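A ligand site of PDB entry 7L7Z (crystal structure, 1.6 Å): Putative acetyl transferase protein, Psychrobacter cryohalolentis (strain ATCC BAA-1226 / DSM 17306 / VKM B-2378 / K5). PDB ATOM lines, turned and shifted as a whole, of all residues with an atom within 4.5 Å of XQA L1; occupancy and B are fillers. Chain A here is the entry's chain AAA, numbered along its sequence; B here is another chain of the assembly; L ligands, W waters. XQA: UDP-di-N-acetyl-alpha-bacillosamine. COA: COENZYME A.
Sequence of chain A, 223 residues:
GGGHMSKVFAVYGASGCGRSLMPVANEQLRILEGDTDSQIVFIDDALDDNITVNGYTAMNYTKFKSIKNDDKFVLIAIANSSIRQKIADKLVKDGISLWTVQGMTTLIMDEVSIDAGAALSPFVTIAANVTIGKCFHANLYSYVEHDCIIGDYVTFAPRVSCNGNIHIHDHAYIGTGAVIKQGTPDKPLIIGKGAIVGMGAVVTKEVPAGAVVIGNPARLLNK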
ATOM      1  N   TYR A  12      -7.921  16.373  27.965  1.00  0.00           N
ATOM      2  CA  TYR A  12      -8.987  16.590  26.971  1.00  0.00           C
ATOM      3  C   TYR A  12     -10.148  15.664  27.328  1.00  0.00           C
ATOM      4  O   TYR A  12      -9.979  14.445  27.265  1.00  0.00           O
ATOM      5  CB  TYR A  12      -8.441  16.352  25.564  1.00  0.00           C
ATOM      6  CG  TYR A  12      -9.163  17.108  24.456  1.00  0.00           C
ATOM      7  CD1 TYR A  12     -10.537  17.201  24.397  1.00  0.00           C
ATOM      8  CD2 TYR A  12      -8.431  17.614  23.394  1.00  0.00           C
ATOM      9  CE1 TYR A  12     -11.176  17.888  23.372  1.00  0.00           C
ATOM     10  CE2 TYR A  12      -9.049  18.277  22.339  1.00  0.00           C
ATOM     11  CZ  TYR A  12     -10.427  18.411  22.330  1.00  0.00           C
ATOM     12  OH  TYR A  12     -11.047  19.074  21.306  1.00  0.00           O
ATOM     13  N   GLY A  13     -11.261  16.246  27.787  1.00  0.00           N
ATOM     14  CA  GLY A  13     -12.421  15.541  28.329  1.00  0.00           C
ATOM     15  C   GLY A  13     -12.567  15.804  29.811  1.00  0.00           C
ATOM     16  O   GLY A  13     -11.651  15.489  30.579  1.00  0.00           O
ATOM     17  N   ALA A  14     -13.656  16.450  30.205  1.00  0.00           N
ATOM     18  CA  ALA A  14     -13.901  16.832  31.610  1.00  0.00           C
ATOM     19  C   ALA A  14     -15.099  16.058  32.146  1.00  0.00           C
ATOM     20  O   ALA A  14     -15.645  16.468  33.177  1.00  0.00           O
ATOM     21  CB  ALA A  14     -14.065  18.325  31.687  1.00  0.00           C
ATOM     22  N   SER A  15     -15.478  14.947  31.494  1.00  0.00           N
ATOM     23  CA  SER A  15     -16.540  14.063  32.025  1.00  0.00           C
ATOM     24  C   SER A  15     -15.890  12.992  32.913  1.00  0.00           C
ATOM     25  O   SER A  15     -14.810  13.281  33.461  1.00  0.00           O
ATOM     26  CB  SER A  15     -17.420  13.538  30.907  1.00  0.00           C
ATOM     27  OG  SER A  15     -18.285  14.568  30.463  1.00  0.00           O
ATOM     28  N   GLY A  16     -16.512  11.833  33.062  1.00  0.00           N
ATOM     29  CA  GLY A  16     -16.042  10.847  34.053  1.00  0.00           C
ATOM     30  C   GLY A  16     -14.619  10.409  33.790  1.00  0.00           C
ATOM     31  O   GLY A  16     -13.824  10.334  34.757  1.00  0.00           O
ATOM     32  N   CYS A  17     -14.263  10.137  32.533  1.00  0.00           N
ATOM     33  CA  CYS A  17     -12.904   9.666  32.175  1.00  0.00           C
ATOM     34  C   CYS A  17     -11.875  10.720  32.609  1.00  0.00           C
ATOM     35  O   CYS A  17     -10.895  10.410  33.303  1.00  0.00           O
ATOM     36  CB  CYS A  17     -12.835   9.405  30.676  1.00  0.00           C
ATOM     37  SG  CYS A  17     -11.227   8.750  30.188  1.00  0.00           S
ATOM     38  N   GLY A  18     -12.101  11.973  32.224  1.00  0.00           N
ATOM     39  CA  GLY A  18     -11.170  13.074  32.480  1.00  0.00           C
ATOM     40  C   GLY A  18     -11.068  13.405  33.969  1.00  0.00           C
ATOM     41  O   GLY A  18      -9.972  13.700  34.426  1.00  0.00           O
ATOM     42  N   ILE A  43      -9.557  20.571  28.707  1.00  0.00           N
ATOM     43  CA  ILE A  43     -10.255  20.952  27.447  1.00  0.00           C
ATOM     44  C   ILE A  43     -11.570  20.188  27.369  1.00  0.00           C
ATOM     45  O   ILE A  43     -11.570  18.953  27.490  1.00  0.00           O
ATOM     46  CB  ILE A  43      -9.335  20.656  26.272  1.00  0.00           C
ATOM     47  CG1 ILE A  43      -7.960  21.298  26.456  1.00  0.00           C
ATOM     48  CG2 ILE A  43      -9.984  21.109  24.968  1.00  0.00           C
ATOM     49  CD1 ILE A  43      -6.912  20.671  25.607  1.00  0.00           C
ATOM     50  N   ASP A  44     -12.668  20.872  27.085  1.00  0.00           N
ATOM     51  CA  ASP A  44     -13.895  20.130  26.750  1.00  0.00           C
ATOM     52  C   ASP A  44     -14.718  20.983  25.788  1.00  0.00           C
ATOM     53  O   ASP A  44     -15.054  22.113  26.173  1.00  0.00           O
ATOM     54  CB  ASP A  44     -14.667  19.759  27.998  1.00  0.00           C
ATOM     55  CG  ASP A  44     -15.667  18.677  27.710  1.00  0.00           C
ATOM     56  OD1 ASP A  44     -15.456  17.561  28.203  1.00  0.00           O
ATOM     57  OD2 ASP A  44     -16.627  18.942  26.916  1.00  0.00           O
ATOM     58  N   ASP A  45     -15.036  20.435  24.621  1.00  0.00           N
ATOM     59  CA  ASP A  45     -15.730  21.203  23.548  1.00  0.00           C
ATOM     60  C   ASP A  45     -17.220  21.389  23.855  1.00  0.00           C
ATOM     61  O   ASP A  45     -17.894  22.108  23.083  1.00  0.00           O
ATOM     62  CB  ASP A  45     -15.495  20.562  22.195  1.00  0.00           C
ATOM     63  CG  ASP A  45     -14.023  20.462  21.866  1.00  0.00           C
ATOM     64  OD1 ASP A  45     -13.581  19.365  21.493  1.00  0.00           O
ATOM     65  OD2 ASP A  45     -13.342  21.510  21.988  1.00  0.00           O
ATOM     66  N   ALA A  46     -17.727  20.884  24.967  1.00  0.00           N
ATOM     67  CA  ALA A  46     -19.094  21.179  25.428  1.00  0.00           C
ATOM     68  C   ALA A  46     -19.123  22.598  25.972  1.00  0.00           C
ATOM     69  O   ALA A  46     -20.211  23.140  26.182  1.00  0.00           O
ATOM     70  CB  ALA A  46     -19.537  20.170  26.462  1.00  0.00           C
ATOM     71  N   ALA A  77      -8.521  12.075  27.429  1.00  0.00           N
ATOM     72  CA  ALA A  77      -9.283  11.299  28.437  1.00  0.00           C
ATOM     73  C   ALA A  77     -10.721  11.179  27.934  1.00  0.00           C
ATOM     74  O   ALA A  77     -11.649  11.644  28.621  1.00  0.00           O
ATOM     75  CB  ALA A  77      -9.248  11.970  29.764  1.00  0.00           C
ATOM     76  N   ILE A  78     -10.860  10.567  26.765  1.00  0.00           N
ATOM     77  CA  ILE A  78     -12.173  10.208  26.184  1.00  0.00           C
ATOM     78  C   ILE A  78     -12.062   8.738  25.800  1.00  0.00           C
ATOM     79  O   ILE A  78     -11.144   8.388  25.057  1.00  0.00           O
ATOM     80  CB  ILE A  78     -12.538  11.107  24.996  1.00  0.00           C
ATOM     81  CG1 ILE A  78     -12.709  12.572  25.422  1.00  0.00           C
ATOM     82  CG2 ILE A  78     -13.782  10.564  24.306  1.00  0.00           C
ATOM     83  CD1 ILE A  78     -12.600  13.552  24.272  1.00  0.00           C
ATOM     84  N   ALA A  79     -12.915   7.919  26.388  1.00  0.00           N
ATOM     85  CA  ALA A  79     -12.776   6.447  26.328  1.00  0.00           C
ATOM     86  C   ALA A  79     -13.157   5.958  24.923  1.00  0.00           C
ATOM     87  O   ALA A  79     -12.616   4.944  24.472  1.00  0.00           O
ATOM     88  CB  ALA A  79     -13.614   5.808  27.400  1.00  0.00           C
ATOM     89  N   ILE A  83     -13.480   8.749  18.748  1.00  0.00           N
ATOM     90  CA  ILE A  83     -13.289  10.187  19.137  1.00  0.00           C
ATOM     91  C   ILE A  83     -11.806  10.392  19.479  1.00  0.00           C
ATOM     92  O   ILE A  83     -11.195  11.393  19.068  1.00  0.00           O
ATOM     93  CB  ILE A  83     -14.211  10.595  20.302  1.00  0.00           C
ATOM     94  CG1 ILE A  83     -15.691  10.429  19.947  1.00  0.00           C
ATOM     95  CG2 ILE A  83     -13.897  12.008  20.763  1.00  0.00           C
ATOM     96  CD1 ILE A  83     -16.628  10.932  21.017  1.00  0.00           C
ATOM     97  N   ILE A  87      -9.419  13.250  17.735  1.00  0.00           N
ATOM     98  CA  ILE A  87      -8.776  14.337  18.532  1.00  0.00           C
ATOM     99  C   ILE A  87      -7.244  14.239  18.431  1.00  0.00           C
ATOM    100  O   ILE A  87      -6.598  15.271  18.222  1.00  0.00           O
ATOM    101  CB  ILE A  87      -9.279  14.294  19.976  1.00  0.00           C
ATOM    102  CG1 ILE A  87     -10.746  14.719  20.026  1.00  0.00           C
ATOM    103  CG2 ILE A  87      -8.387  15.166  20.875  1.00  0.00           C
ATOM    104  CD1 ILE A  87     -11.415  14.432  21.316  1.00  0.00           C
ATOM    105  N   ASN A 139      -7.326   1.543  32.255  1.00  0.00           N
ATOM    106  CA  ASN A 139      -8.044   2.048  33.437  1.00  0.00           C
ATOM    107  C   ASN A 139      -7.593   1.270  34.669  1.00  0.00           C
ATOM    108  O   ASN A 139      -6.856   0.272  34.564  1.00  0.00           O
ATOM    109  CB  ASN A 139      -9.561   2.043  33.220  1.00  0.00           C
ATOM    110  CG  ASN A 139     -10.289   3.207  33.870  1.00  0.00           C
ATOM    111  OD1 ASN A 139      -9.922   3.659  34.960  1.00  0.00           O
ATOM    112  ND2 ASN A 139     -11.413   3.575  33.254  1.00  0.00           N
ATOM    113  N   GLU B 145     -16.257   4.619  41.359  1.00  0.00           N
ATOM    114  CA  GLU B 145     -15.838   5.529  40.286  1.00  0.00           C
ATOM    115  C   GLU B 145     -16.759   6.766  40.263  1.00  0.00           C
ATOM    116  O   GLU B 145     -17.631   6.948  41.152  1.00  0.00           O
ATOM    117  CB  GLU B 145     -15.718   4.763  38.974  1.00  0.00           C
ATOM    118  CG  GLU B 145     -14.275   4.557  38.548  1.00  0.00           C
ATOM    119  CD  GLU B 145     -13.598   5.798  37.981  1.00  0.00           C
ATOM    120  OE1 GLU B 145     -12.449   5.691  37.533  1.00  0.00           O
ATOM    121  OE2 GLU B 145     -14.224   6.873  37.969  1.00  0.00           O
ATOM    122  N   HIS B 146     -16.508   7.603  39.276  1.00  0.00           N
ATOM    123  CA  HIS B 146     -16.967   9.008  39.228  1.00  0.00           C
ATOM    124  C   HIS B 146     -18.469   9.117  39.494  1.00  0.00           C
ATOM    125  O   HIS B 146     -19.283   8.349  38.947  1.00  0.00           O
ATOM    126  CB  HIS B 146     -16.573   9.607  37.867  1.00  0.00           C
ATOM    127  CG  HIS B 146     -17.252   8.969  36.702  1.00  0.00           C
ATOM    128  ND1 HIS B 146     -18.451   9.441  36.199  1.00  0.00           N
ATOM    129  CD2 HIS B 146     -16.923   7.904  35.938  1.00  0.00           C
ATOM    130  CE1 HIS B 146     -18.815   8.691  35.169  1.00  0.00           C
ATOM    131  NE2 HIS B 146     -17.891   7.756  34.983  1.00  0.00           N
ATOM    132  N   ASN B 163     -18.574   1.041  38.979  1.00  0.00           N
ATOM    133  CA  ASN B 163     -18.303   2.027  37.910  1.00  0.00           C
ATOM    134  C   ASN B 163     -19.073   3.317  38.180  1.00  0.00           C
ATOM    135  O   ASN B 163     -19.684   3.465  39.265  1.00  0.00           O
ATOM    136  CB  ASN B 163     -18.612   1.395  36.567  1.00  0.00           C
ATOM    137  CG  ASN B 163     -17.530   0.428  36.183  1.00  0.00           C
ATOM    138  OD1 ASN B 163     -16.357   0.777  36.278  1.00  0.00           O
ATOM    139  ND2 ASN B 163     -17.910  -0.746  35.713  1.00  0.00           N
ATOM    140  N   GLY B 164     -19.034   4.232  37.208  1.00  0.00           N
ATOM    141  CA  GLY B 164     -19.556   5.583  37.418  1.00  0.00           C
ATOM    142  C   GLY B 164     -21.074   5.660  37.445  1.00  0.00           C
ATOM    143  O   GLY B 164     -21.731   4.799  36.904  1.00  0.00           O
ATOM    144  N   GLN B 182     -21.801   0.924  34.654  1.00  0.00           N
ATOM    145  CA  GLN B 182     -21.999   2.377  34.883  1.00  0.00           C
ATOM    146  C   GLN B 182     -23.465   2.733  34.562  1.00  0.00           C
ATOM    147  O   GLN B 182     -24.047   2.138  33.625  1.00  0.00           O
ATOM    148  CB  GLN B 182     -21.013   3.177  34.048  1.00  0.00           C
ATOM    149  CG  GLN B 182     -21.364   3.263  32.563  1.00  0.00           C
ATOM    150  CD  GLN B 182     -20.798   2.158  31.703  1.00  0.00           C
ATOM    151  OE1 GLN B 182     -20.349   1.111  32.166  1.00  0.00           O
ATOM    152  NE2 GLN B 182     -20.831   2.392  30.395  1.00  0.00           N
HETATM  153  O74 XQA L   1     -17.605   4.115  34.500  1.00  0.00           O
HETATM  154  C74 XQA L   1     -16.468   4.565  34.451  1.00  0.00           C
HETATM  155  C84 XQA L   1     -15.560   4.251  35.606  1.00  0.00           C
HETATM  156  N4A XQA L   1     -15.842   5.303  33.494  1.00  0.00           N
HETATM  157  C4' XQA L   1     -16.293   5.641  32.153  1.00  0.00           C
HETATM  158  C3' XQA L   1     -17.482   6.595  32.150  1.00  0.00           C
HETATM  159  O3' XQA L   1     -18.617   6.184  32.954  1.00  0.00           O
HETATM  160  C5' XQA L   1     -15.145   6.284  31.280  1.00  0.00           C
HETATM  161  C6' XQA L   1     -13.801   5.574  31.086  1.00  0.00           C
HETATM  162  O5' XQA L   1     -15.601   6.465  29.928  1.00  0.00           O
HETATM  163  C1' XQA L   1     -16.784   7.224  29.822  1.00  0.00           C
HETATM  164  C2' XQA L   1     -17.913   6.709  30.695  1.00  0.00           C
HETATM  165  N2' XQA L   1     -19.067   7.575  30.524  1.00  0.00           N
HETATM  166  C7' XQA L   1     -20.263   7.072  30.184  1.00  0.00           C
HETATM  167  C8' XQA L   1     -21.435   8.038  30.157  1.00  0.00           C
HETATM  168  O7' XQA L   1     -20.379   5.870  29.945  1.00  0.00           O
HETATM  169  O1' XQA L   1     -16.449   8.534  30.217  1.00  0.00           O
HETATM  170  PB  XQA L   1     -16.015   9.577  29.067  1.00  0.00           P
HETATM  171  O2B XQA L   1     -15.637  10.740  29.903  1.00  0.00           O
HETATM  172  O1B XQA L   1     -15.089   8.966  28.026  1.00  0.00           O
HETATM  173  O3A XQA L   1     -17.393   9.703  28.223  1.00  0.00           O
HETATM  174  PA  XQA L   1     -18.458  10.852  28.185  1.00  0.00           P
HETATM  175  O2A XQA L   1     -19.399  10.657  27.014  1.00  0.00           O
HETATM  176  O1A XQA L   1     -19.170  10.852  29.507  1.00  0.00           O
HETATM  177  O5B XQA L   1     -17.664  12.228  27.980  1.00  0.00           O
HETATM  178  C5B XQA L   1     -16.797  12.573  26.913  1.00  0.00           C
HETATM  179  C4B XQA L   1     -16.419  14.049  27.075  1.00  0.00           C
HETATM  180  C2B XQA L   1     -17.591  15.005  27.089  1.00  0.00           C
HETATM  181  O3B XQA L   1     -17.548  15.931  28.188  1.00  0.00           O
HETATM  182  C3B XQA L   1     -17.472  15.685  25.753  1.00  0.00           C
HETATM  183  O2' XQA L   1     -17.983  17.014  25.735  1.00  0.00           O
HETATM  184  C1B XQA L   1     -15.991  15.609  25.475  1.00  0.00           C
HETATM  185  O4B XQA L   1     -15.609  14.319  25.940  1.00  0.00           O
HETATM  186  N1  XQA L   1     -15.682  15.732  24.063  1.00  0.00           N
HETATM  187  C2  XQA L   1     -14.934  16.837  23.625  1.00  0.00           C
HETATM  188  O2  XQA L   1     -14.540  17.718  24.421  1.00  0.00           O
HETATM  189  C6  XQA L   1     -16.116  14.776  23.195  1.00  0.00           C
HETATM  190  C5  XQA L   1     -15.843  14.950  21.824  1.00  0.00           C
HETATM  191  C4  XQA L   1     -15.102  16.052  21.405  1.00  0.00           C
HETATM  192  O4  XQA L   1     -14.832  16.210  20.170  1.00  0.00           O
HETATM  193  N3  XQA L   1     -14.702  16.994  22.279  1.00  0.00           N
HETATM  194  N1A COA L   2     -22.234  -9.797  30.459  1.00  0.00           N
HETATM  195  C2A COA L   2     -23.362 -10.496  30.321  1.00  0.00           C
HETATM  196  N3A COA L   2     -24.561 -10.080  29.903  1.00  0.00           N
HETATM  197  C4A COA L   2     -24.526  -8.785  29.569  1.00  0.00           C
HETATM  198  C5A COA L   2     -23.436  -7.943  29.635  1.00  0.00           C
HETATM  199  C6A COA L   2     -22.238  -8.482  30.114  1.00  0.00           C
HETATM  200  N6A COA L   2     -21.101  -7.780  30.202  1.00  0.00           N
HETATM  201  N7A COA L   2     -23.777  -6.657  29.205  1.00  0.00           N
HETATM  202  C8A COA L   2     -25.055  -6.751  28.884  1.00  0.00           C
HETATM  203  N9A COA L   2     -25.560  -8.017  29.086  1.00  0.00           N
HETATM  204  C1B COA L   2     -26.923  -8.489  28.854  1.00  0.00           C
HETATM  205  C2B COA L   2     -27.987  -7.520  29.386  1.00  0.00           C
HETATM  206  O2B COA L   2     -28.342  -7.812  30.725  1.00  0.00           O
HETATM  207  C3B COA L   2     -29.125  -7.728  28.368  1.00  0.00           C
HETATM  208  O3B COA L   2     -29.889  -8.896  28.669  1.00  0.00           O
HETATM  209  P3B COA L   2     -31.461  -8.825  28.198  1.00  0.00           P
HETATM  210  O7A COA L   2     -32.115  -7.672  28.938  1.00  0.00           O
HETATM  211  O8A COA L   2     -31.531  -8.650  26.681  1.00  0.00           O
HETATM  212  O9A COA L   2     -32.016 -10.173  28.648  1.00  0.00           O
HETATM  213  C4B COA L   2     -28.331  -7.892  27.065  1.00  0.00           C
HETATM  214  O4B COA L   2     -27.125  -8.585  27.451  1.00  0.00           O
HETATM  215  C5B COA L   2     -27.966  -6.599  26.373  1.00  0.00           C
HETATM  216  O5B COA L   2     -27.879  -5.545  27.374  1.00  0.00           O
HETATM  217  P1A COA L   2     -27.483  -4.051  26.971  1.00  0.00           P
HETATM  218  O1A COA L   2     -27.014  -3.306  28.179  1.00  0.00           O
HETATM  219  O2A COA L   2     -28.585  -3.465  26.158  1.00  0.00           O
HETATM  220  O3A COA L   2     -26.203  -4.313  26.042  1.00  0.00           O
HETATM  221  P2A COA L   2     -25.376  -3.357  25.050  1.00  0.00           P
HETATM  222  O4A COA L   2     -25.365  -3.995  23.693  1.00  0.00           O
HETATM  223  O5A COA L   2     -25.838  -1.951  25.218  1.00  0.00           O
HETATM  224  O6A COA L   2     -23.893  -3.473  25.653  1.00  0.00           O
HETATM  225  CBP COA L   2     -21.910  -4.626  26.370  1.00  0.00           C
HETATM  226  CCP COA L   2     -23.283  -4.782  25.743  1.00  0.00           C
HETATM  227  CDP COA L   2     -21.009  -3.811  25.432  1.00  0.00           C
HETATM  228  CEP COA L   2     -21.302  -6.016  26.563  1.00  0.00           C
HETATM  229  CAP COA L   2     -22.025  -3.892  27.721  1.00  0.00           C
HETATM  230  OAP COA L   2     -23.035  -4.389  28.607  1.00  0.00           O
HETATM  231  C9P COA L   2     -20.676  -3.939  28.418  1.00  0.00           C
HETATM  232  O9P COA L   2     -20.300  -5.001  28.938  1.00  0.00           O
HETATM  233  N8P COA L   2     -19.981  -2.813  28.419  1.00  0.00           N
HETATM  234  C7P COA L   2     -18.870  -2.533  29.323  1.00  0.00           C
HETATM  235  C6P COA L   2     -19.275  -1.741  30.579  1.00  0.00           C
HETATM  236  C5P COA L   2     -17.996  -1.356  31.316  1.00  0.00           C
HETATM  237  O5P COA L   2     -16.990  -2.046  31.175  1.00  0.00           O
HETATM  238  N4P COA L   2     -17.982  -0.208  32.016  1.00  0.00           N
HETATM  239  C3P COA L   2     -16.759   0.395  32.548  1.00  0.00           C
HETATM  240  C2P COA L   2     -16.692   1.889  32.319  1.00  0.00           C
HETATM  241  S1P COA L   2     -15.157   2.582  32.994  1.00  0.00           S
HETATM  242  O   HOH W   1     -21.722   9.908  26.171  1.00  0.00           O
HETATM  243  O   HOH W   2     -20.712  16.824  26.405  1.00  0.00           O
HETATM  244  O   HOH W   3     -20.290   7.747  26.639  1.00  0.00           O
HETATM  245  O   HOH W   4     -18.720  10.196  32.062  1.00  0.00           O
HETATM  246  O   HOH W   5     -16.280   3.949  29.254  1.00  0.00           O
HETATM  247  O   HOH W   6     -22.946   4.813  29.515  1.00  0.00           O
HETATM  248  O   HOH W   7     -16.179   8.455  25.828  1.00  0.00           O
HETATM  249  O   HOH W   8     -13.940  14.931  17.825  1.00  0.00           O
HETATM  250  O   HOH W   9     -21.496  11.571  30.462  1.00  0.00           O
HETATM  251  O   HOH W  10     -10.846   5.073  29.765  1.00  0.00           O
HETATM  252  O   HOH W  11     -17.992   9.872  24.564  1.00  0.00           O
HETATM  253  O   HOH W  12     -20.073  13.130  25.336  1.00  0.00           O
HETATM  254  O   HOH W  13     -13.928  12.771  29.912  1.00  0.00           O
HETATM  255  O   HOH W  14     -21.385   7.084  33.351  1.00  0.00           O
HETATM  256  O   HOH W  15     -13.544  18.639  18.688  1.00  0.00           O
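OG of Ser 15 lies within hydrogen-bond range of O3B of XQA L1 (2.8 Å). N of Asp 45 is in hydrogen-bond range of O2 of XQA L1 (2.8 Å). N of Ala 79 lies within hydrogen-bond range of O1B of XQA L1. OD1 of Asp 45 is in hydrogen-bond range of N3 of XQA L1, at 2.7 Å. N of Gly 16 sits at hydrogen-bond distance from O2B of XQA L1, 3.5 Å away. A ring nitrogen (NE2) of His 146 of chain B sits at hydrogen-bond distance from an oxygen (O3') of XQA L1 (2.7 Å). The backbone NH (N) of Gly 164 of chain B sits at hydrogen-bond distance from an oxygen (O74) of XQA L1 (3.1 Å). OD2 of Asp 44 is in hydrogen-bond range of O2' of XQA L1, at 2.6 Å. N4P of COA L2 sits at hydrogen-bond distance from OE1 of Gln 182 of chain B, at 2.7 Å. N of Cys 17 lies within hydrogen-bond range of O2B of XQA L1, at 3.0 Å.
S1P of COA L2 sits close to N4A of XQA L1 (2.9 Å).
The side-chain carboxylate (OD1) of Asp 44 is in hydrogen-bond range of the backbone NH (N) of Ala 14, at 2.9 Å. The side-chain sulfur (SG) of Cys 17 sits close to the backbone carbonyl oxygen (O) of Ala 77 (3.3 Å). The backbone carbonyl oxygen of Tyr 12 lies within hydrogen-bond range of the backbone NH of Ala 77 (2.8 Å). OD1 of Asp 45 sits at hydrogen-bond distance from OH of Tyr 12, 2.6 Å away. OD2 of Asp 44 sits at hydrogen-bond distance from N of Ala 46 (3.0 Å).
Tyr 12 touches XQA L1. CB of Ala 46 touches O2' of XQA L1 (3.6 Å). Ile 78 touches XQA L1. Ile 83 touches XQA L1. Asn 139 touches XQA L1. Glu 145 of chain B touches XQA L1. Asn 163 of chain B touches XQA L1 (CB to O74, 3.6 Å). Gln 182 of chain B touches XQA L1 (NE2 to O7', 3.5 Å). Hydrophobic or aromatic side chains within 4 Å of XQA L1: Tyr 12, Ala 46, Ile 78, Ala 79, Ile 83 and His 146 of chain B. The nearest printed residue that does not touch XQA L1 is Ile 87 (4.02 Å).
Water W7 lies within hydrogen-bond range of O1B of XQA L1 (2.5 Å) and N of Ala 79 (3.4 Å). Water W13 lies within hydrogen-bond range of an oxygen (O2B) of XQA L1, the backbone carbonyl oxygen (O) of Ala 77, the backbone NH (N) of Gly 18 and the backbone NH (N) of Ser 15. Water W4 bridges an oxygen (O1A) of XQA L1 (2.7 Å) and the backbone NH (N) of Gly 16 (2.9 Å). Water W6 lies within hydrogen-bond range of an oxygen (O7') of XQA L1 (2.8 Å) and the side-chain amide nitrogen (NE2) of Gln 182 of chain B (3.3 Å). Water W15 bridges OD1 of Asp 45 (2.9 Å) and O4 of XQA L1 (3.1 Å).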
